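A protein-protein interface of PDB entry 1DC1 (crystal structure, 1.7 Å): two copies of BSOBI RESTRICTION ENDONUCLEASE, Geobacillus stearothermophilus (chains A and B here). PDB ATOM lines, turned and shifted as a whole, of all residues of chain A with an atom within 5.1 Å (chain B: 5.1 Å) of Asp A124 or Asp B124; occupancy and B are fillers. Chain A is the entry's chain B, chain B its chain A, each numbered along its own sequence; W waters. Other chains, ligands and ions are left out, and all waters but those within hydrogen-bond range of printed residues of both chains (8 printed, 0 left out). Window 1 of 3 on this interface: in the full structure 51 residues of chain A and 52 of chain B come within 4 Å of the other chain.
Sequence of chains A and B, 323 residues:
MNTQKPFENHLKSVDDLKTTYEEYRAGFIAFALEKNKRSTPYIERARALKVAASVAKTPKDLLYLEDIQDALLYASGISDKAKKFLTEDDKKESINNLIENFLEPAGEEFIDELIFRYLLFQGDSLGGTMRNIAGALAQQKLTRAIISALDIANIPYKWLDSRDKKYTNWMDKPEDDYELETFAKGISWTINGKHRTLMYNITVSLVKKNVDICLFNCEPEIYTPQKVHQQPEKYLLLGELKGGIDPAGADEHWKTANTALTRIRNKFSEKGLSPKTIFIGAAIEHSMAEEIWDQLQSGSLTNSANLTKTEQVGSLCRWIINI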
ATOM      1  N   TYR A  74      24.249  13.074 -24.923  1.00  0.00           N
ATOM      2  CA  TYR A  74      24.258  14.337 -24.226  1.00  0.00           C
ATOM      3  C   TYR A  74      23.123  15.257 -24.673  1.00  0.00           C
ATOM      4  O   TYR A  74      22.428  15.843 -23.831  1.00  0.00           O
ATOM      5  CB  TYR A  74      25.614  15.043 -24.388  1.00  0.00           C
ATOM      6  CG  TYR A  74      25.962  15.875 -23.149  1.00  0.00           C
ATOM      7  CD1 TYR A  74      25.335  17.120 -22.918  1.00  0.00           C
ATOM      8  CD2 TYR A  74      26.842  15.386 -22.166  1.00  0.00           C
ATOM      9  CE1 TYR A  74      25.570  17.862 -21.720  1.00  0.00           C
ATOM     10  CE2 TYR A  74      27.081  16.110 -20.991  1.00  0.00           C
ATOM     11  CZ  TYR A  74      26.424  17.348 -20.789  1.00  0.00           C
ATOM     12  OH  TYR A  74      26.586  18.039 -19.635  1.00  0.00           O
ATOM     13  N   LEU A 120      22.791  23.622 -25.783  1.00  0.00           N
ATOM     14  CA  LEU A 120      21.988  23.982 -24.648  1.00  0.00           C
ATOM     15  C   LEU A 120      22.362  23.121 -23.416  1.00  0.00           C
ATOM     16  O   LEU A 120      22.520  23.667 -22.333  1.00  0.00           O
ATOM     17  CB  LEU A 120      20.503  23.780 -24.974  1.00  0.00           C
ATOM     18  CG  LEU A 120      19.556  24.128 -23.818  1.00  0.00           C
ATOM     19  CD1 LEU A 120      19.659  25.663 -23.624  1.00  0.00           C
ATOM     20  CD2 LEU A 120      18.101  23.627 -24.099  1.00  0.00           C
ATOM     21  N   PHE A 121      22.451  21.791 -23.572  1.00  0.00           N
ATOM     22  CA  PHE A 121      22.802  20.938 -22.426  1.00  0.00           C
ATOM     23  C   PHE A 121      24.306  21.036 -22.075  1.00  0.00           C
ATOM     24  O   PHE A 121      24.674  21.007 -20.903  1.00  0.00           O
ATOM     25  CB  PHE A 121      22.352  19.472 -22.669  1.00  0.00           C
ATOM     26  CG  PHE A 121      20.840  19.307 -22.790  1.00  0.00           C
ATOM     27  CD1 PHE A 121      19.979  19.964 -21.918  1.00  0.00           C
ATOM     28  CD2 PHE A 121      20.298  18.609 -23.830  1.00  0.00           C
ATOM     29  CE1 PHE A 121      18.596  19.935 -22.109  1.00  0.00           C
ATOM     30  CE2 PHE A 121      18.933  18.573 -24.024  1.00  0.00           C
ATOM     31  CZ  PHE A 121      18.078  19.233 -23.177  1.00  0.00           C
ATOM     32  N   GLN A 122      25.169  21.194 -23.077  1.00  0.00           N
ATOM     33  CA  GLN A 122      26.617  21.344 -22.837  1.00  0.00           C
ATOM     34  C   GLN A 122      26.887  22.659 -22.045  1.00  0.00           C
ATOM     35  O   GLN A 122      27.890  22.790 -21.373  1.00  0.00           O
ATOM     36  CB  GLN A 122      27.376  21.356 -24.171  1.00  0.00           C
ATOM     37  CG  GLN A 122      27.654  19.954 -24.704  1.00  0.00           C
ATOM     38  CD  GLN A 122      28.777  19.236 -23.946  1.00  0.00           C
ATOM     39  OE1 GLN A 122      28.602  18.131 -23.416  1.00  0.00           O
ATOM     40  NE2 GLN A 122      29.936  19.862 -23.894  1.00  0.00           N
ATOM     41  N   GLY A 123      25.990  23.635 -22.135  1.00  0.00           N
ATOM     42  CA  GLY A 123      26.179  24.860 -21.381  1.00  0.00           C
ATOM     43  C   GLY A 123      26.218  24.590 -19.881  1.00  0.00           C
ATOM     44  O   GLY A 123      26.895  25.287 -19.133  1.00  0.00           O
ATOM     45  N   ASP A 124      25.488  23.577 -19.419  1.00  0.00           N
ATOM     46  CA  ASP A 124      25.494  23.266 -17.979  1.00  0.00           C
ATOM     47  C   ASP A 124      26.856  22.618 -17.657  1.00  0.00           C
ATOM     48  O   ASP A 124      27.375  22.771 -16.555  1.00  0.00           O
ATOM     49  CB  ASP A 124      24.343  22.310 -17.648  1.00  0.00           C
ATOM     50  CG  ASP A 124      23.763  22.507 -16.225  1.00  0.00           C
ATOM     51  OD1 ASP A 124      24.279  23.278 -15.401  1.00  0.00           O
ATOM     52  OD2 ASP A 124      22.750  21.865 -15.946  1.00  0.00           O
ATOM     53  N   SER A 125      27.418  21.896 -18.623  1.00  0.00           N
ATOM     54  CA  SER A 125      28.755  21.285 -18.447  1.00  0.00           C
ATOM     55  C   SER A 125      29.832  22.384 -18.348  1.00  0.00           C
ATOM     56  O   SER A 125      30.711  22.291 -17.477  1.00  0.00           O
ATOM     57  CB  SER A 125      29.111  20.349 -19.618  1.00  0.00           C
ATOM     58  OG  SER A 125      30.462  19.951 -19.523  1.00  0.00           O
ATOM     59  N   LEU A 126      29.774  23.396 -19.239  1.00  0.00           N
ATOM     60  CA  LEU A 126      30.715  24.509 -19.188  1.00  0.00           C
ATOM     61  C   LEU A 126      30.555  25.198 -17.837  1.00  0.00           C
ATOM     62  O   LEU A 126      31.532  25.492 -17.215  1.00  0.00           O
ATOM     63  CB  LEU A 126      30.503  25.516 -20.334  1.00  0.00           C
ATOM     64  CG  LEU A 126      31.318  26.832 -20.197  1.00  0.00           C
ATOM     65  CD1 LEU A 126      32.807  26.581 -20.214  1.00  0.00           C
ATOM     66  CD2 LEU A 126      30.949  27.794 -21.282  1.00  0.00           C
ATOM     67  N   GLY A 127      29.319  25.432 -17.392  1.00  0.00           N
ATOM     68  CA  GLY A 127      29.060  26.025 -16.088  1.00  0.00           C
ATOM     69  C   GLY A 127      29.735  25.234 -14.975  1.00  0.00           C
ATOM     70  O   GLY A 127      30.353  25.842 -14.097  1.00  0.00           O
ATOM     71  N   GLY A 128      29.644  23.898 -15.024  1.00  0.00           N
ATOM     72  CA  GLY A 128      30.291  23.037 -14.047  1.00  0.00           C
ATOM     73  C   GLY A 128      31.798  23.212 -14.064  1.00  0.00           C
ATOM     74  O   GLY A 128      32.425  23.344 -13.010  1.00  0.00           O
ATOM     75  N   ARG A 131      32.864  26.563 -12.436  1.00  0.00           N
ATOM     76  CA  ARG A 131      32.806  26.566 -10.960  1.00  0.00           C
ATOM     77  C   ARG A 131      34.103  25.932 -10.394  1.00  0.00           C
ATOM     78  O   ARG A 131      34.681  26.434  -9.457  1.00  0.00           O
ATOM     79  CB  ARG A 131      31.506  25.838 -10.500  1.00  0.00           C
ATOM     80  CG  ARG A 131      30.212  26.684 -10.885  1.00  0.00           C
ATOM     81  CD  ARG A 131      28.894  25.897 -10.654  1.00  0.00           C
ATOM     82  NE  ARG A 131      27.649  26.692 -10.748  1.00  0.00           N
ATOM     83  CZ  ARG A 131      27.239  27.294 -11.866  1.00  0.00           C
ATOM     84  NH1 ARG A 131      27.955  27.215 -12.959  1.00  0.00           N
ATOM     85  NH2 ARG A 131      26.067  27.881 -11.930  1.00  0.00           N
ATOM     86  N   TYR B  74      23.572  38.244 -23.338  1.00  0.00           N
ATOM     87  CA  TYR B  74      23.659  36.882 -22.818  1.00  0.00           C
ATOM     88  C   TYR B  74      24.678  36.037 -23.590  1.00  0.00           C
ATOM     89  O   TYR B  74      25.518  35.352 -22.977  1.00  0.00           O
ATOM     90  CB  TYR B  74      22.282  36.178 -22.849  1.00  0.00           C
ATOM     91  CG  TYR B  74      22.116  35.196 -21.689  1.00  0.00           C
ATOM     92  CD1 TYR B  74      22.751  33.930 -21.718  1.00  0.00           C
ATOM     93  CD2 TYR B  74      21.443  35.587 -20.515  1.00  0.00           C
ATOM     94  CE1 TYR B  74      22.735  33.073 -20.594  1.00  0.00           C
ATOM     95  CE2 TYR B  74      21.418  34.737 -19.377  1.00  0.00           C
ATOM     96  CZ  TYR B  74      22.078  33.481 -19.420  1.00  0.00           C
ATOM     97  OH  TYR B  74      22.145  32.680 -18.287  1.00  0.00           O
ATOM     98  N   LEU B 120      24.692  27.932 -25.688  1.00  0.00           N
ATOM     99  CA  LEU B 120      25.682  27.454 -24.754  1.00  0.00           C
ATOM    100  C   LEU B 120      25.552  28.158 -23.387  1.00  0.00           C
ATOM    101  O   LEU B 120      25.556  27.511 -22.351  1.00  0.00           O
ATOM    102  CB  LEU B 120      27.076  27.680 -25.310  1.00  0.00           C
ATOM    103  CG  LEU B 120      28.209  27.109 -24.435  1.00  0.00           C
ATOM    104  CD1 LEU B 120      28.123  25.598 -24.368  1.00  0.00           C
ATOM    105  CD2 LEU B 120      29.573  27.567 -25.043  1.00  0.00           C
ATOM    106  N   PHE B 121      25.439  29.483 -23.372  1.00  0.00           N
ATOM    107  CA  PHE B 121      25.311  30.206 -22.104  1.00  0.00           C
ATOM    108  C   PHE B 121      23.893  30.038 -21.487  1.00  0.00           C
ATOM    109  O   PHE B 121      23.752  29.904 -20.291  1.00  0.00           O
ATOM    110  CB  PHE B 121      25.708  31.680 -22.327  1.00  0.00           C
ATOM    111  CG  PHE B 121      27.178  31.850 -22.646  1.00  0.00           C
ATOM    112  CD1 PHE B 121      28.141  31.123 -21.939  1.00  0.00           C
ATOM    113  CD2 PHE B 121      27.606  32.665 -23.695  1.00  0.00           C
ATOM    114  CE1 PHE B 121      29.522  31.201 -22.278  1.00  0.00           C
ATOM    115  CE2 PHE B 121      28.996  32.737 -24.028  1.00  0.00           C
ATOM    116  CZ  PHE B 121      29.929  32.008 -23.322  1.00  0.00           C
ATOM    117  N   GLN B 122      22.866  30.010 -22.329  1.00  0.00           N
ATOM    118  CA  GLN B 122      21.514  29.824 -21.883  1.00  0.00           C
ATOM    119  C   GLN B 122      21.382  28.402 -21.220  1.00  0.00           C
ATOM    120  O   GLN B 122      20.492  28.176 -20.386  1.00  0.00           O
ATOM    121  CB  GLN B 122      20.559  29.974 -23.086  1.00  0.00           C
ATOM    122  CG  GLN B 122      20.118  31.397 -23.362  1.00  0.00           C
ATOM    123  CD  GLN B 122      19.136  31.956 -22.318  1.00  0.00           C
ATOM    124  OE1 GLN B 122      19.456  32.906 -21.624  1.00  0.00           O
ATOM    125  NE2 GLN B 122      17.968  31.382 -22.218  1.00  0.00           N
ATOM    126  N   GLY B 123      22.263  27.462 -21.568  1.00  0.00           N
ATOM    127  CA  GLY B 123      22.197  26.152 -20.943  1.00  0.00           C
ATOM    128  C   GLY B 123      22.419  26.211 -19.432  1.00  0.00           C
ATOM    129  O   GLY B 123      21.886  25.406 -18.673  1.00  0.00           O
ATOM    130  N   ASP B 124      23.214  27.171 -18.976  1.00  0.00           N
ATOM    131  CA  ASP B 124      23.463  27.306 -17.549  1.00  0.00           C
ATOM    132  C   ASP B 124      22.198  27.925 -16.912  1.00  0.00           C
ATOM    133  O   ASP B 124      21.878  27.682 -15.734  1.00  0.00           O
ATOM    134  CB  ASP B 124      24.722  28.169 -17.335  1.00  0.00           C
ATOM    135  CG  ASP B 124      25.500  27.808 -16.051  1.00  0.00           C
ATOM    136  OD1 ASP B 124      25.087  26.907 -15.310  1.00  0.00           O
ATOM    137  OD2 ASP B 124      26.525  28.454 -15.797  1.00  0.00           O
ATOM    138  N   SER B 125      21.478  28.734 -17.689  1.00  0.00           N
ATOM    139  CA  SER B 125      20.220  29.306 -17.202  1.00  0.00           C
ATOM    140  C   SER B 125      19.175  28.205 -17.026  1.00  0.00           C
ATOM    141  O   SER B 125      18.448  28.200 -16.035  1.00  0.00           O
ATOM    142  CB  SER B 125      19.661  30.330 -18.184  1.00  0.00           C
ATOM    143  OG  SER B 125      18.433  30.833 -17.691  1.00  0.00           O
ATOM    144  N   LEU B 126      19.076  27.289 -17.993  1.00  0.00           N
ATOM    145  CA  LEU B 126      18.141  26.170 -17.898  1.00  0.00           C
ATOM    146  C   LEU B 126      18.540  25.294 -16.718  1.00  0.00           C
ATOM    147  O   LEU B 126      17.661  24.823 -15.993  1.00  0.00           O
ATOM    148  CB  LEU B 126      18.089  25.344 -19.193  1.00  0.00           C
ATOM    149  CG  LEU B 126      17.390  23.965 -19.074  1.00  0.00           C
ATOM    150  CD1 LEU B 126      15.913  24.173 -18.833  1.00  0.00           C
ATOM    151  CD2 LEU B 126      17.596  23.157 -20.289  1.00  0.00           C
ATOM    152  N   GLY B 127      19.843  25.088 -16.521  1.00  0.00           N
ATOM    153  CA  GLY B 127      20.311  24.322 -15.376  1.00  0.00           C
ATOM    154  C   GLY B 127      19.821  24.979 -14.078  1.00  0.00           C
ATOM    155  O   GLY B 127      19.324  24.265 -13.174  1.00  0.00           O
ATOM    156  N   GLY B 128      19.938  26.318 -13.978  1.00  0.00           N
ATOM    157  CA  GLY B 128      19.465  27.082 -12.813  1.00  0.00           C
ATOM    158  C   GLY B 128      17.971  26.863 -12.551  1.00  0.00           C
ATOM    159  O   GLY B 128      17.493  26.559 -11.435  1.00  0.00           O
ATOM    160  N   ARG B 131      17.182  23.370 -11.183  1.00  0.00           N
ATOM    161  CA  ARG B 131      17.520  23.134  -9.782  1.00  0.00           C
ATOM    162  C   ARG B 131      16.365  23.648  -8.916  1.00  0.00           C
ATOM    163  O   ARG B 131      15.965  22.998  -7.953  1.00  0.00           O
ATOM    164  CB  ARG B 131      18.886  23.778  -9.483  1.00  0.00           C
ATOM    165  CG  ARG B 131      20.071  22.968 -10.161  1.00  0.00           C
ATOM    166  CD  ARG B 131      21.408  23.755 -10.075  1.00  0.00           C
ATOM    167  NE  ARG B 131      22.658  23.045 -10.447  1.00  0.00           N
ATOM    168  CZ  ARG B 131      22.873  22.463 -11.631  1.00  0.00           C
ATOM    169  NH1 ARG B 131      21.952  22.462 -12.575  1.00  0.00           N
ATOM    170  NH2 ARG B 131      24.056  22.006 -11.925  1.00  0.00           N
HETATM  171  O   HOH W   1      23.059  25.379 -13.883  1.00  0.00           O
HETATM  172  O   HOH W   2      26.194  23.998 -11.780  1.00  0.00           O
HETATM  173  O   HOH W   3      26.614  24.877 -14.244  1.00  0.00           O
HETATM  174  O   HOH W   4      28.386  29.555 -14.329  1.00  0.00           O
HETATM  175  O   HOH W   5      23.918  26.068 -11.437  1.00  0.00           O
HETATM  176  O   HOH W   6      27.231  27.871 -20.035  1.00  0.00           O
HETATM  177  O   HOH W   7      20.864  20.800 -14.307  1.00  0.00           O
HETATM  178  O   HOH W   8      21.406  22.963 -19.808  1.00  0.00           O
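NH1 of Arg B131 lies within salt-bridge range of OD2 of Asp A124, at 3.5 Å.
The side-chain carboxylate of Asp B124 lies within salt-bridge range of the guanidinium group of Arg A131 (3.4 Å).
O of Gly A127 is in hydrogen-bond range of NH1 of Arg A131 (3.0 Å).
The backbone carbonyl oxygen (O) of Gly B127 sits at hydrogen-bond distance from the guanidinium group (NH1) of Arg B131.
Leu A120 touches Gly B123.
Leu A120 touches Leu B126.
CD2 of Leu B126 touches CE1 of Phe A121, 3.8 Å away.
Gln A122 touches Leu B120 (C to CD1, 3.9 Å).
CA of Gly A123 touches O of Leu B120 (2.9 Å).
Asp A124 touches Asp B124.
Asp A124 touches Gly B127.
Phe B121 touches Leu A126 (CE1 to CD2, 3.8 Å).
CA of Gly A127 touches OD2 of Asp B124, at 3.5 Å.
Asp A124 touches three residues of chain B.
Of chain A, only Asp A124 (3.7 Å), Gly A127 (3.5 Å) and Arg A131 (3.4 Å) come within 4 Å of Asp B124.
Of the printed residues of chain B, Gln A122 touches Leu B120 (3.9 Å).
Of the printed residues of chain B, Leu A126 touches Phe B121.
Ser B125 touches none of the printed residues of chain A.
The nearest residue of chain B that does not touch Asp A124 is Gly B123 (4.04 Å).
The nearest residue of chain A that does not touch Asp B124 is Gly A123 (4.03 Å).
Printed residues of chain B that touch a printed residue of chain A: Leu B120, Phe B121, Gly B123, Asp B124, Leu B126, Gly B127 and Arg B131.
Among the printed residues, 11 pairs touch across the chains.
Phe A121 touches Leu B126, and with the chains exchanged Leu A126 touches Phe B121.
Asp B124 touches its own counterpart, Asp A124.
Asp A124 touches Gly B127, and with the chains exchanged Gly A127 touches Asp B124.
Asp A124 touches Arg B131, and with the chains exchanged Arg A131 touches Asp B124.
Of the 11 pairs that touch across the chains among the printed residues, 9 have their exchanged pair printed and touching as well.
Water W8 lies within hydrogen-bond range of the backbone carbonyl oxygen (O) of Gly B123 (2.7 Å) and the backbone carbonyl oxygen (O) of Leu A120 (2.8 Å).
Water W3 lies within hydrogen-bond range of OD1 of Asp B124 (2.8 Å), NH1 of Arg A131 (3.0 Å), OD1 of Asp A124 (3.1 Å) and N of Gly A128 (3.3 Å).
Water W6 lies within hydrogen-bond range of the backbone carbonyl oxygen of Gly A123 and the backbone carbonyl oxygen of Leu B120.
Water W5 bridges the guanidinium group (NH2) of Arg A131 (2.9 Å) and the guanidinium group (NE) of Arg B131 (3.4 Å).
Water W1 lies within hydrogen-bond range of the side-chain carboxylate of Asp A124 (2.9 Å), the side-chain carboxylate of Asp B124 (2.9 Å), the backbone NH of Gly B128 (3.3 Å) and the guanidinium group of Arg B131 (3.4 Å).
Water W2 bridges the guanidinium group (NH2) of Arg B131 and the guanidinium group (NE) of Arg A131.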
